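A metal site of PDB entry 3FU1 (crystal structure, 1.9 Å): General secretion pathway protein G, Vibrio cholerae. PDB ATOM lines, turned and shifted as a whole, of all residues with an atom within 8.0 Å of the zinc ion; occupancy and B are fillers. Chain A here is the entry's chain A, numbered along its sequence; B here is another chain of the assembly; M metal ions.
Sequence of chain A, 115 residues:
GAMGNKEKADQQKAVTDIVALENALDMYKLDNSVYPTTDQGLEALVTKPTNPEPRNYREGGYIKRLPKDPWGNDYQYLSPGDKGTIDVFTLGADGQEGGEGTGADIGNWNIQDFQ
The side-chain carboxylate (OD1) of Asp 26 lies within hydrogen-bond range of the side-chain hydroxyl (OH) of Tyr 35 (2.8 Å). The side-chain carboxylate of Glu 22 is in hydrogen-bond range of the side-chain amide nitrogen of Asn 108 (3.1 Å). The side-chain amide nitrogen (NE2) of Gln 115 of chain B lies within hydrogen-bond range of the backbone carbonyl oxygen (O) of Asn 108 (2.9 Å).
Three residues have an atom within 4 Å of the zinc ion: Glu 22, Asp 26 and Gln 115 of chain B.
The zinc ion is bound by the chain-end carboxylate of Gln 115 of chain B, the side-chain carboxylate of Glu 22 and the side-chain carboxylate of Asp 26. Slightly farther from the zinc ion lies O of Gln 115 of chain B (2.8 Å).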
ATOM      1  N   VAL A  19      26.378  30.350 -21.243  1.00  0.00           N
ATOM      2  CA  VAL A  19      26.583  30.631 -22.652  1.00  0.00           C
ATOM      3  C   VAL A  19      27.182  29.423 -23.362  1.00  0.00           C
ATOM      4  O   VAL A  19      26.720  29.050 -24.438  1.00  0.00           O
ATOM      5  CB  VAL A  19      27.438  31.897 -22.851  1.00  0.00           C
ATOM      6  CG1 VAL A  19      27.933  31.975 -24.282  1.00  0.00           C
ATOM      7  CG2 VAL A  19      26.625  33.115 -22.432  1.00  0.00           C
ATOM      8  N   LEU A  21      27.112  26.215 -22.351  1.00  0.00           N
ATOM      9  CA  LEU A  21      26.084  25.180 -22.339  1.00  0.00           C
ATOM     10  C   LEU A  21      25.019  25.375 -23.427  1.00  0.00           C
ATOM     11  O   LEU A  21      24.703  24.427 -24.169  1.00  0.00           O
ATOM     12  CB  LEU A  21      25.434  25.080 -20.949  1.00  0.00           C
ATOM     13  CG  LEU A  21      26.322  24.481 -19.849  1.00  0.00           C
ATOM     14  CD1 LEU A  21      25.698  24.643 -18.458  1.00  0.00           C
ATOM     15  CD2 LEU A  21      26.595  23.008 -20.151  1.00  0.00           C
ATOM     16  N   GLU A  22      24.457  26.576 -23.522  1.00  0.00           N
ATOM     17  CA  GLU A  22      23.492  26.837 -24.587  1.00  0.00           C
ATOM     18  C   GLU A  22      24.127  26.705 -25.967  1.00  0.00           C
ATOM     19  O   GLU A  22      23.483  26.177 -26.890  1.00  0.00           O
ATOM     20  CB  GLU A  22      22.782  28.184 -24.450  1.00  0.00           C
ATOM     21  CG  GLU A  22      21.984  28.516 -25.742  1.00  0.00           C
ATOM     22  CD  GLU A  22      20.853  29.501 -25.570  1.00  0.00           C
ATOM     23  OE1 GLU A  22      20.650  30.055 -24.474  1.00  0.00           O
ATOM     24  OE2 GLU A  22      20.161  29.735 -26.599  1.00  0.00           O
ATOM     25  N   ASN A  23      25.356  27.177 -26.129  1.00  0.00           N
ATOM     26  CA  ASN A  23      26.075  26.956 -27.389  1.00  0.00           C
ATOM     27  C   ASN A  23      26.137  25.470 -27.716  1.00  0.00           C
ATOM     28  O   ASN A  23      25.859  25.099 -28.875  1.00  0.00           O
ATOM     29  CB  ASN A  23      27.487  27.554 -27.375  1.00  0.00           C
ATOM     30  CG  ASN A  23      27.488  29.068 -27.447  1.00  0.00           C
ATOM     31  OD1 ASN A  23      26.440  29.701 -27.600  1.00  0.00           O
ATOM     32  ND2 ASN A  23      28.679  29.664 -27.348  1.00  0.00           N
ATOM     33  N   ALA A  24      26.500  24.625 -26.746  1.00  0.00           N
ATOM     34  CA  ALA A  24      26.565  23.180 -26.983  1.00  0.00           C
ATOM     35  C   ALA A  24      25.190  22.575 -27.325  1.00  0.00           C
ATOM     36  O   ALA A  24      25.078  21.733 -28.213  1.00  0.00           O
ATOM     37  CB  ALA A  24      27.198  22.454 -25.796  1.00  0.00           C
ATOM     38  N   LEU A  25      24.157  22.984 -26.609  1.00  0.00           N
ATOM     39  CA  LEU A  25      22.782  22.554 -26.871  1.00  0.00           C
ATOM     40  C   LEU A  25      22.310  22.967 -28.281  1.00  0.00           C
ATOM     41  O   LEU A  25      21.666  22.185 -28.964  1.00  0.00           O
ATOM     42  CB  LEU A  25      21.827  23.114 -25.813  1.00  0.00           C
ATOM     43  CG  LEU A  25      22.037  22.487 -24.432  1.00  0.00           C
ATOM     44  CD1 LEU A  25      21.636  23.431 -23.315  1.00  0.00           C
ATOM     45  CD2 LEU A  25      21.320  21.126 -24.319  1.00  0.00           C
ATOM     46  N   ASP A  26      22.639  24.193 -28.688  1.00  0.00           N
ATOM     47  CA  ASP A  26      22.286  24.689 -30.026  1.00  0.00           C
ATOM     48  C   ASP A  26      22.970  23.894 -31.134  1.00  0.00           C
ATOM     49  O   ASP A  26      22.360  23.656 -32.187  1.00  0.00           O
ATOM     50  CB  ASP A  26      22.615  26.176 -30.160  1.00  0.00           C
ATOM     51  CG  ASP A  26      21.705  27.058 -29.339  1.00  0.00           C
ATOM     52  OD1 ASP A  26      20.620  26.564 -28.931  1.00  0.00           O
ATOM     53  OD2 ASP A  26      22.063  28.244 -29.114  1.00  0.00           O
ATOM     54  N   MET A  27      24.213  23.504 -30.907  1.00  0.00           N
ATOM     55  CA  MET A  27      24.928  22.622 -31.845  1.00  0.00           C
ATOM     56  C   MET A  27      24.355  21.228 -31.865  1.00  0.00           C
ATOM     57  O   MET A  27      24.277  20.605 -32.932  1.00  0.00           O
ATOM     58  CB  MET A  27      26.416  22.543 -31.498  1.00  0.00           C
ATOM     59  CG  MET A  27      27.239  23.619 -32.167  1.00  0.00           C
ATOM     60  SD  MET A  27      27.345  23.508 -33.985  1.00  0.00           S
ATOM     61  CE  MET A  27      28.580  24.791 -34.194  1.00  0.00           C
ATOM     62  N   TYR A  35      16.414  19.454 -29.425  1.00  0.00           N
ATOM     63  CA  TYR A  35      17.200  19.579 -28.228  1.00  0.00           C
ATOM     64  C   TYR A  35      17.101  18.303 -27.427  1.00  0.00           C
ATOM     65  O   TYR A  35      16.101  17.565 -27.548  1.00  0.00           O
ATOM     66  CB  TYR A  35      16.674  20.717 -27.354  1.00  0.00           C
ATOM     67  CG  TYR A  35      17.006  22.100 -27.838  1.00  0.00           C
ATOM     68  CD1 TYR A  35      18.326  22.526 -27.938  1.00  0.00           C
ATOM     69  CD2 TYR A  35      15.989  23.009 -28.165  1.00  0.00           C
ATOM     70  CE1 TYR A  35      18.634  23.811 -28.363  1.00  0.00           C
ATOM     71  CE2 TYR A  35      16.298  24.284 -28.609  1.00  0.00           C
ATOM     72  CZ  TYR A  35      17.618  24.687 -28.702  1.00  0.00           C
ATOM     73  OH  TYR A  35      17.896  25.954 -29.139  1.00  0.00           O
ATOM     74  N   ILE A  86      14.617  26.515 -24.566  1.00  0.00           N
ATOM     75  CA  ILE A  86      15.365  25.836 -23.531  1.00  0.00           C
ATOM     76  C   ILE A  86      15.716  26.773 -22.376  1.00  0.00           C
ATOM     77  O   ILE A  86      16.021  27.961 -22.577  1.00  0.00           O
ATOM     78  CB  ILE A  86      16.664  25.175 -24.054  1.00  0.00           C
ATOM     79  CG1 ILE A  86      17.487  26.142 -24.908  1.00  0.00           C
ATOM     80  CG2 ILE A  86      16.311  23.905 -24.836  1.00  0.00           C
ATOM     81  CD1 ILE A  86      19.000  25.771 -25.019  1.00  0.00           C
ATOM     82  N   ASN A 108      19.756  31.547 -18.881  1.00  0.00           N
ATOM     83  CA  ASN A 108      19.939  32.064 -20.243  1.00  0.00           C
ATOM     84  C   ASN A 108      18.955  33.198 -20.594  1.00  0.00           C
ATOM     85  O   ASN A 108      19.312  34.107 -21.364  1.00  0.00           O
ATOM     86  CB  ASN A 108      19.959  30.936 -21.294  1.00  0.00           C
ATOM     87  CG  ASN A 108      18.714  30.045 -21.293  1.00  0.00           C
ATOM     88  OD1 ASN A 108      17.956  29.988 -20.330  1.00  0.00           O
ATOM     89  ND2 ASN A 108      18.527  29.313 -22.397  1.00  0.00           N
ATOM     90  N   LYS B   8      27.600  28.663 -37.795  1.00  0.00           N
ATOM     91  CA  LYS B   8      27.112  28.604 -36.414  1.00  0.00           C
ATOM     92  C   LYS B   8      28.278  28.717 -35.444  1.00  0.00           C
ATOM     93  O   LYS B   8      28.207  29.467 -34.461  1.00  0.00           O
ATOM     94  CB  LYS B   8      26.351  27.307 -36.156  1.00  0.00           C
ATOM     95  CG  LYS B   8      25.814  27.149 -34.732  1.00  0.00           C
ATOM     96  CD  LYS B   8      24.927  28.298 -34.303  1.00  0.00           C
ATOM     97  CE  LYS B   8      23.621  28.368 -35.081  1.00  0.00           C
ATOM     98  NZ  LYS B   8      22.977  29.716 -34.960  1.00  0.00           N
ATOM     99  N   GLN B  11      29.405  32.365 -35.239  1.00  0.00           N
ATOM    100  CA  GLN B  11      28.473  33.072 -34.373  1.00  0.00           C
ATOM    101  C   GLN B  11      28.734  32.766 -32.899  1.00  0.00           C
ATOM    102  O   GLN B  11      28.736  33.676 -32.056  1.00  0.00           O
ATOM    103  CB  GLN B  11      27.030  32.723 -34.739  1.00  0.00           C
ATOM    104  CG  GLN B  11      25.990  33.239 -33.760  1.00  0.00           C
ATOM    105  CD  GLN B  11      24.595  32.740 -34.064  1.00  0.00           C
ATOM    106  OE1 GLN B  11      24.207  32.628 -35.231  1.00  0.00           O
ATOM    107  NE2 GLN B  11      23.825  32.447 -33.003  1.00  0.00           N
ATOM    108  N   GLN B  12      28.930  31.485 -32.584  1.00  0.00           N
ATOM    109  CA  GLN B  12      29.125  31.079 -31.190  1.00  0.00           C
ATOM    110  C   GLN B  12      30.431  31.562 -30.601  1.00  0.00           C
ATOM    111  O   GLN B  12      30.486  31.907 -29.420  1.00  0.00           O
ATOM    112  CB  GLN B  12      29.028  29.561 -31.041  1.00  0.00           C
ATOM    113  CG  GLN B  12      27.597  29.089 -31.225  1.00  0.00           C
ATOM    114  CD  GLN B  12      27.422  27.618 -30.986  1.00  0.00           C
ATOM    115  OE1 GLN B  12      28.400  26.876 -30.872  1.00  0.00           O
ATOM    116  NE2 GLN B  12      26.179  27.182 -30.910  1.00  0.00           N
ATOM    117  N   ILE B 111      23.429  40.421 -27.916  1.00  0.00           N
ATOM    118  CA  ILE B 111      23.825  39.019 -27.719  1.00  0.00           C
ATOM    119  C   ILE B 111      22.616  38.094 -27.585  1.00  0.00           C
ATOM    120  O   ILE B 111      22.711  36.919 -27.932  1.00  0.00           O
ATOM    121  CB  ILE B 111      24.748  38.831 -26.473  1.00  0.00           C
ATOM    122  CG1 ILE B 111      26.162  39.361 -26.742  1.00  0.00           C
ATOM    123  CG2 ILE B 111      24.888  37.360 -26.113  1.00  0.00           C
ATOM    124  CD1 ILE B 111      26.927  38.644 -27.828  1.00  0.00           C
ATOM    125  N   GLN B 112      21.491  38.634 -27.097  1.00  0.00           N
ATOM    126  CA  GLN B 112      20.244  37.878 -26.935  1.00  0.00           C
ATOM    127  C   GLN B 112      19.770  37.299 -28.273  1.00  0.00           C
ATOM    128  O   GLN B 112      19.160  36.212 -28.321  1.00  0.00           O
ATOM    129  CB  GLN B 112      19.146  38.775 -26.334  1.00  0.00           C
ATOM    130  CG  GLN B 112      19.330  39.121 -24.849  1.00  0.00           C
ATOM    131  CD  GLN B 112      20.588  39.941 -24.559  1.00  0.00           C
ATOM    132  OE1 GLN B 112      20.965  40.819 -25.336  1.00  0.00           O
ATOM    133  NE2 GLN B 112      21.244  39.631 -23.441  1.00  0.00           N
ATOM    134  N   ASP B 113      20.044  38.007 -29.364  1.00  0.00           N
ATOM    135  CA  ASP B 113      19.665  37.534 -30.701  1.00  0.00           C
ATOM    136  C   ASP B 113      20.567  36.423 -31.230  1.00  0.00           C
ATOM    137  O   ASP B 113      20.245  35.793 -32.241  1.00  0.00           O
ATOM    138  CB  ASP B 113      19.659  38.686 -31.713  1.00  0.00           C
ATOM    139  CG  ASP B 113      18.702  39.803 -31.339  1.00  0.00           C
ATOM    140  OD1 ASP B 113      17.556  39.508 -30.919  1.00  0.00           O
ATOM    141  OD2 ASP B 113      19.077  40.980 -31.488  1.00  0.00           O
ATOM    142  N   PHE B 114      21.722  36.195 -30.583  1.00  0.00           N
ATOM    143  CA  PHE B 114      22.693  35.203 -31.053  1.00  0.00           C
ATOM    144  C   PHE B 114      23.055  34.125 -30.020  1.00  0.00           C
ATOM    145  O   PHE B 114      23.840  33.232 -30.329  1.00  0.00           O
ATOM    146  CB  PHE B 114      23.952  35.916 -31.542  1.00  0.00           C
ATOM    147  CG  PHE B 114      23.701  36.905 -32.639  1.00  0.00           C
ATOM    148  CD1 PHE B 114      23.708  36.506 -33.969  1.00  0.00           C
ATOM    149  CD2 PHE B 114      23.409  38.228 -32.346  1.00  0.00           C
ATOM    150  CE1 PHE B 114      23.457  37.422 -34.998  1.00  0.00           C
ATOM    151  CE2 PHE B 114      23.167  39.143 -33.364  1.00  0.00           C
ATOM    152  CZ  PHE B 114      23.184  38.734 -34.703  1.00  0.00           C
ATOM    153  N   GLN B 115      22.449  34.192 -28.837  1.00  0.00           N
ATOM    154  CA  GLN B 115      22.699  33.228 -27.747  1.00  0.00           C
ATOM    155  C   GLN B 115      22.395  31.768 -28.127  1.00  0.00           C
ATOM    156  O   GLN B 115      23.125  30.875 -27.690  1.00  0.00           O
ATOM    157  CB  GLN B 115      21.845  33.555 -26.528  1.00  0.00           C
ATOM    158  CG  GLN B 115      22.443  34.485 -25.531  1.00  0.00           C
ATOM    159  CD  GLN B 115      21.449  34.792 -24.418  1.00  0.00           C
ATOM    160  OE1 GLN B 115      20.954  35.914 -24.309  1.00  0.00           O
ATOM    161  NE2 GLN B 115      21.119  33.791 -23.603  1.00  0.00           N
ATOM    162  OXT GLN B 115      21.416  31.450 -28.812  1.00  0.00           O
HETATM  163 ZN    ZN M   1      20.704  29.629 -28.527  1.00  0.00          ZN
